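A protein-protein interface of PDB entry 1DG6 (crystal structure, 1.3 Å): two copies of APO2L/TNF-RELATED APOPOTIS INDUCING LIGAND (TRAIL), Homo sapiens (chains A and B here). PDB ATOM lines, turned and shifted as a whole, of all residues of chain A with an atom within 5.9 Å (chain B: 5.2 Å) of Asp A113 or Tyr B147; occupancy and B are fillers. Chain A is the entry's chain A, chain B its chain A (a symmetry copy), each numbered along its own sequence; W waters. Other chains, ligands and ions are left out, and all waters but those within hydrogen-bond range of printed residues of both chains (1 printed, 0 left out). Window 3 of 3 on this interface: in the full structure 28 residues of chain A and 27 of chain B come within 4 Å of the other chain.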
ATOM      1  N   LYS A 111     -28.777  18.591 -26.805  1.00  0.00           N
ATOM      2  CA  LYS A 111     -29.143  17.266 -26.248  1.00  0.00           C
ATOM      3  C   LYS A 111     -28.014  16.569 -25.498  1.00  0.00           C
ATOM      4  O   LYS A 111     -28.242  15.681 -24.646  1.00  0.00           O
ATOM      5  CB  LYS A 111     -29.701  16.502 -27.450  1.00  0.00           C
ATOM      6  CG  LYS A 111     -30.154  15.094 -27.143  1.00  0.00           C
ATOM      7  CD  LYS A 111     -31.250  14.671 -28.105  1.00  0.00           C
ATOM      8  CE  LYS A 111     -30.852  13.327 -28.699  1.00  0.00           C
ATOM      9  NZ  LYS A 111     -31.155  13.269 -30.149  1.00  0.00           N
ATOM     10  N   ASN A 112     -26.795  16.945 -25.786  1.00  0.00           N
ATOM     11  CA  ASN A 112     -25.474  16.671 -25.287  1.00  0.00           C
ATOM     12  C   ASN A 112     -25.100  15.238 -24.941  1.00  0.00           C
ATOM     13  O   ASN A 112     -24.200  15.050 -24.097  1.00  0.00           O
ATOM     14  CB  ASN A 112     -25.227  17.540 -24.008  1.00  0.00           C
ATOM     15  CG  ASN A 112     -24.934  18.922 -24.588  1.00  0.00           C
ATOM     16  OD1 ASN A 112     -24.427  18.935 -25.718  1.00  0.00           O
ATOM     17  ND2 ASN A 112     -25.264  19.979 -23.879  1.00  0.00           N
ATOM     18  N   ASP A 113     -25.738  14.261 -25.577  1.00  0.00           N
ATOM     19  CA  ASP A 113     -25.402  12.870 -25.288  1.00  0.00           C
ATOM     20  C   ASP A 113     -24.011  12.523 -25.798  1.00  0.00           C
ATOM     21  O   ASP A 113     -23.620  12.882 -26.894  1.00  0.00           O
ATOM     22  CB  ASP A 113     -26.415  11.903 -25.930  1.00  0.00           C
ATOM     23  CG  ASP A 113     -26.667  12.194 -27.396  1.00  0.00           C
ATOM     24  OD1 ASP A 113     -27.031  13.360 -27.732  1.00  0.00           O
ATOM     25  OD2 ASP A 113     -26.528  11.269 -28.243  1.00  0.00           O
ATOM     26  N   LYS A 114     -23.278  11.768 -24.974  1.00  0.00           N
ATOM     27  CA  LYS A 114     -21.946  11.393 -25.371  1.00  0.00           C
ATOM     28  C   LYS A 114     -21.851   9.871 -25.460  1.00  0.00           C
ATOM     29  O   LYS A 114     -22.294   9.188 -24.528  1.00  0.00           O
ATOM     30  CB  LYS A 114     -20.920  11.900 -24.338  1.00  0.00           C
ATOM     31  CG  LYS A 114     -20.787  13.429 -24.346  1.00  0.00           C
ATOM     32  CD  LYS A 114     -20.065  13.900 -23.081  1.00  0.00           C
ATOM     33  CE  LYS A 114     -19.901  15.393 -23.034  1.00  0.00           C
ATOM     34  NZ  LYS A 114     -21.179  16.136 -22.808  1.00  0.00           N
ATOM     35  N   GLN A 115     -21.243   9.405 -26.571  1.00  0.00           N
ATOM     36  CA  GLN A 115     -20.799   8.016 -26.678  1.00  0.00           C
ATOM     37  C   GLN A 115     -19.316   7.959 -26.381  1.00  0.00           C
ATOM     38  O   GLN A 115     -18.525   8.459 -27.180  1.00  0.00           O
ATOM     39  CB  GLN A 115     -21.069   7.526 -28.105  1.00  0.00           C
ATOM     40  CG  GLN A 115     -22.565   7.602 -28.419  1.00  0.00           C
ATOM     41  CD  GLN A 115     -22.873   7.035 -29.796  1.00  0.00           C
ATOM     42  OE1 GLN A 115     -24.047   6.871 -30.164  1.00  0.00           O
ATOM     43  NE2 GLN A 115     -21.834   6.761 -30.550  1.00  0.00           N
ATOM     44  N   ASN A 138     -22.507   5.383 -22.434  1.00  0.00           N
ATOM     45  CA  ASN A 138     -23.171   6.654 -22.695  1.00  0.00           C
ATOM     46  C   ASN A 138     -23.165   7.534 -21.450  1.00  0.00           C
ATOM     47  O   ASN A 138     -23.163   7.007 -20.339  1.00  0.00           O
ATOM     48  CB  ASN A 138     -24.629   6.481 -23.165  1.00  0.00           C
ATOM     49  CG  ASN A 138     -25.515   5.847 -22.134  1.00  0.00           C
ATOM     50  OD1 ASN A 138     -25.567   4.641 -21.927  1.00  0.00           O
ATOM     51  ND2 ASN A 138     -26.244   6.680 -21.370  1.00  0.00           N
ATOM     52  N   SER A 139     -23.180   8.852 -21.630  1.00  0.00           N
ATOM     53  CA  SER A 139     -23.252   9.750 -20.465  1.00  0.00           C
ATOM     54  C   SER A 139     -24.688   9.814 -19.980  1.00  0.00           C
ATOM     55  O   SER A 139     -25.655   9.520 -20.697  1.00  0.00           O
ATOM     56  CB  SER A 139     -22.725  11.123 -20.880  1.00  0.00           C
ATOM     57  OG  SER A 139     -23.544  11.607 -21.946  1.00  0.00           O
ATOM     58  N   TRP A 141     -28.275  11.044 -19.217  1.00  0.00           N
ATOM     59  CA  TRP A 141     -29.134  11.885 -20.045  1.00  0.00           C
ATOM     60  C   TRP A 141     -29.823  12.981 -19.278  1.00  0.00           C
ATOM     61  O   TRP A 141     -30.512  13.861 -19.850  1.00  0.00           O
ATOM     62  CB  TRP A 141     -30.204  11.008 -20.707  1.00  0.00           C
ATOM     63  CG  TRP A 141     -29.683  10.062 -21.750  1.00  0.00           C
ATOM     64  CD1 TRP A 141     -29.167   8.795 -21.540  1.00  0.00           C
ATOM     65  CD2 TRP A 141     -29.628  10.284 -23.153  1.00  0.00           C
ATOM     66  NE1 TRP A 141     -28.791   8.214 -22.733  1.00  0.00           N
ATOM     67  CE2 TRP A 141     -29.083   9.143 -23.757  1.00  0.00           C
ATOM     68  CE3 TRP A 141     -30.013  11.354 -23.974  1.00  0.00           C
ATOM     69  CZ2 TRP A 141     -28.902   9.057 -25.141  1.00  0.00           C
ATOM     70  CZ3 TRP A 141     -29.842  11.275 -25.322  1.00  0.00           C
ATOM     71  CH2 TRP A 141     -29.291  10.134 -25.920  1.00  0.00           C
ATOM     72  N   PHE B 102     -28.888  -0.746 -26.260  1.00  0.00           N
ATOM     73  CA  PHE B 102     -30.320  -0.738 -26.532  1.00  0.00           C
ATOM     74  C   PHE B 102     -30.768   0.673 -26.907  1.00  0.00           C
ATOM     75  O   PHE B 102     -30.157   1.640 -26.510  1.00  0.00           O
ATOM     76  CB  PHE B 102     -31.179  -1.210 -25.338  1.00  0.00           C
ATOM     77  CG  PHE B 102     -30.916  -0.492 -24.025  1.00  0.00           C
ATOM     78  CD1 PHE B 102     -31.602   0.666 -23.687  1.00  0.00           C
ATOM     79  CD2 PHE B 102     -29.969  -0.965 -23.117  1.00  0.00           C
ATOM     80  CE1 PHE B 102     -31.362   1.346 -22.513  1.00  0.00           C
ATOM     81  CE2 PHE B 102     -29.719  -0.284 -21.918  1.00  0.00           C
ATOM     82  CZ  PHE B 102     -30.421   0.872 -21.593  1.00  0.00           C
ATOM     83  N   GLN B 103     -31.880   0.715 -27.639  1.00  0.00           N
ATOM     84  CA  GLN B 103     -32.595   1.961 -27.796  1.00  0.00           C
ATOM     85  C   GLN B 103     -33.755   2.006 -26.775  1.00  0.00           C
ATOM     86  O   GLN B 103     -34.312   0.948 -26.443  1.00  0.00           O
ATOM     87  CB  GLN B 103     -33.143   2.119 -29.214  1.00  0.00           C
ATOM     88  CG  GLN B 103     -33.951   3.396 -29.270  1.00  0.00           C
ATOM     89  CD  GLN B 103     -33.328   4.450 -30.172  1.00  0.00           C
ATOM     90  OE1 GLN B 103     -33.184   5.617 -29.770  1.00  0.00           O
ATOM     91  NE2 GLN B 103     -32.985   4.019 -31.387  1.00  0.00           N
ATOM     92  N   GLU B 104     -34.083   3.179 -26.282  1.00  0.00           N
ATOM     93  CA  GLU B 104     -35.078   3.479 -25.275  1.00  0.00           C
ATOM     94  C   GLU B 104     -36.400   3.905 -25.934  1.00  0.00           C
ATOM     95  O   GLU B 104     -36.417   3.977 -27.167  1.00  0.00           O
ATOM     96  CB  GLU B 104     -34.630   4.596 -24.336  1.00  0.00           C
ATOM     97  CG  GLU B 104     -33.704   4.183 -23.217  1.00  0.00           C
ATOM     98  CD  GLU B 104     -34.368   3.445 -22.073  1.00  0.00           C
ATOM     99  OE1 GLU B 104     -35.251   2.602 -22.356  1.00  0.00           O
ATOM    100  OE2 GLU B 104     -33.998   3.684 -20.902  1.00  0.00           O
ATOM    101  N   ALA B 145     -33.657   9.618 -21.691  1.00  0.00           N
ATOM    102  CA  ALA B 145     -32.692   8.640 -22.233  1.00  0.00           C
ATOM    103  C   ALA B 145     -33.197   8.041 -23.533  1.00  0.00           C
ATOM    104  O   ALA B 145     -34.291   7.507 -23.554  1.00  0.00           O
ATOM    105  CB  ALA B 145     -32.436   7.556 -21.203  1.00  0.00           C
ATOM    106  N   GLU B 146     -32.452   8.118 -24.621  1.00  0.00           N
ATOM    107  CA  GLU B 146     -32.879   7.595 -25.923  1.00  0.00           C
ATOM    108  C   GLU B 146     -32.158   6.268 -26.250  1.00  0.00           C
ATOM    109  O   GLU B 146     -32.655   5.539 -27.104  1.00  0.00           O
ATOM    110  CB  GLU B 146     -32.529   8.612 -27.000  1.00  0.00           C
ATOM    111  CG  GLU B 146     -33.230   9.940 -26.805  1.00  0.00           C
ATOM    112  CD  GLU B 146     -33.038  11.005 -27.858  1.00  0.00           C
ATOM    113  OE1 GLU B 146     -32.389  10.720 -28.878  1.00  0.00           O
ATOM    114  OE2 GLU B 146     -33.521  12.152 -27.670  1.00  0.00           O
ATOM    115  N   TYR B 147     -31.022   6.003 -25.605  1.00  0.00           N
ATOM    116  CA  TYR B 147     -30.282   4.753 -25.825  1.00  0.00           C
ATOM    117  C   TYR B 147     -29.367   4.513 -24.603  1.00  0.00           C
ATOM    118  O   TYR B 147     -29.158   5.410 -23.788  1.00  0.00           O
ATOM    119  CB  TYR B 147     -29.469   4.715 -27.134  1.00  0.00           C
ATOM    120  CG  TYR B 147     -28.418   5.798 -27.262  1.00  0.00           C
ATOM    121  CD1 TYR B 147     -27.152   5.725 -26.703  1.00  0.00           C
ATOM    122  CD2 TYR B 147     -28.686   6.952 -28.018  1.00  0.00           C
ATOM    123  CE1 TYR B 147     -26.193   6.710 -26.814  1.00  0.00           C
ATOM    124  CE2 TYR B 147     -27.733   7.946 -28.161  1.00  0.00           C
ATOM    125  CZ  TYR B 147     -26.495   7.836 -27.557  1.00  0.00           C
ATOM    126  OH  TYR B 147     -25.562   8.824 -27.683  1.00  0.00           O
ATOM    127  N   GLY B 148     -28.853   3.280 -24.591  1.00  0.00           N
ATOM    128  CA  GLY B 148     -27.927   2.906 -23.498  1.00  0.00           C
ATOM    129  C   GLY B 148     -26.825   2.028 -24.095  1.00  0.00           C
ATOM    130  O   GLY B 148     -27.064   1.157 -24.917  1.00  0.00           O
ATOM    131  N   LEU B 149     -25.594   2.329 -23.642  1.00  0.00           N
ATOM    132  CA  LEU B 149     -24.367   1.601 -24.010  1.00  0.00           C
ATOM    133  C   LEU B 149     -23.712   1.202 -22.673  1.00  0.00           C
ATOM    134  O   LEU B 149     -23.258   2.137 -21.986  1.00  0.00           O
ATOM    135  CB  LEU B 149     -23.414   2.437 -24.856  1.00  0.00           C
ATOM    136  CG  LEU B 149     -24.014   3.273 -25.973  1.00  0.00           C
ATOM    137  CD1 LEU B 149     -22.870   4.081 -26.608  1.00  0.00           C
ATOM    138  CD2 LEU B 149     -24.674   2.341 -26.974  1.00  0.00           C
HETATM  139  O   HOH W   1     -29.161   4.886 -20.914  1.00  0.00           O
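Among the printed residues, merely in contact across the chains: Gln A115 with Tyr B147, Asn A138 with Gly B148, Trp A141 with Ala B145, Trp A141 with Glu B146, Gln A115 with Leu B149 and Asn A138 with Tyr B147.
NZ of Lys A111 is in salt-bridge range of OE1 of Glu B146.
The backbone carbonyl oxygen (O) of Tyr B147 sits at hydrogen-bond distance from the indole nitrogen (NE1) of Trp A141 (3.0 Å).
The side-chain hydroxyl (OH) of Tyr B147 lies within hydrogen-bond range of the side-chain carboxylate (OD2) of Asp A113 (2.7 Å).
OD1 of Asn A138 sits at hydrogen-bond distance from N of Leu B149, at 2.9 Å.
O of Glu B146 sits at hydrogen-bond distance from N of Glu B104, 2.9 Å away.
The backbone carbonyl oxygen of Phe B102 lies within hydrogen-bond range of the backbone NH of Gly B148.
The indole nitrogen of Trp A141 sits close to the side-chain amide nitrogen of Asn A138 (3.3 Å).
OE1 of Gln B103 lies close to O of Glu B146 (2.7 Å).
No position is printed for both chains.
Of the 10 pairs that touch across the chains among the printed residues, none has its exchanged pair printed and touching as well.
Of chain B, only Tyr B147 comes within 4 Å of Asp A113.
Of chain A, only Asp A113, Gln A115, Asn A138 and Trp A141 come within 4 Å of Tyr B147.
Of the printed residues of chain A, Leu B149 touches Gln A115 and Asn A138.
Of the printed residues of chain B, Asn A138 touches Tyr B147 (3.98 Å), Gly B148 (3.3 Å) and Leu B149 (2.9 Å).
The nearest residue of chain A that does not touch Tyr B147 is Lys A114 (4.5 Å).
Of the 8 printed residues of chain A, 5 touch a printed residue of chain B.
Hydrophobic or aromatic side chains of chain A that line the printed part of chain B: Trp A141.
Printed residues of chain B that touch a printed residue of chain A: Ala B145, Glu B146, Tyr B147, Gly B148 and Leu B149.
Hydrophobic or aromatic side chains of chain B that line the printed part of chain A: Ala B145, Tyr B147 and Leu B149.
Among the printed residues, Asp or Glu carboxylates within 4 Å of a Lys or Arg side-chain nitrogen of the other chain: Lys A111 with Glu B146.
Water W1 lies within hydrogen-bond range of the backbone carbonyl oxygen (O) of Tyr B147 (2.9 Å) and the side-chain amide nitrogen (ND2) of Asn A138 (3.5 Å).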
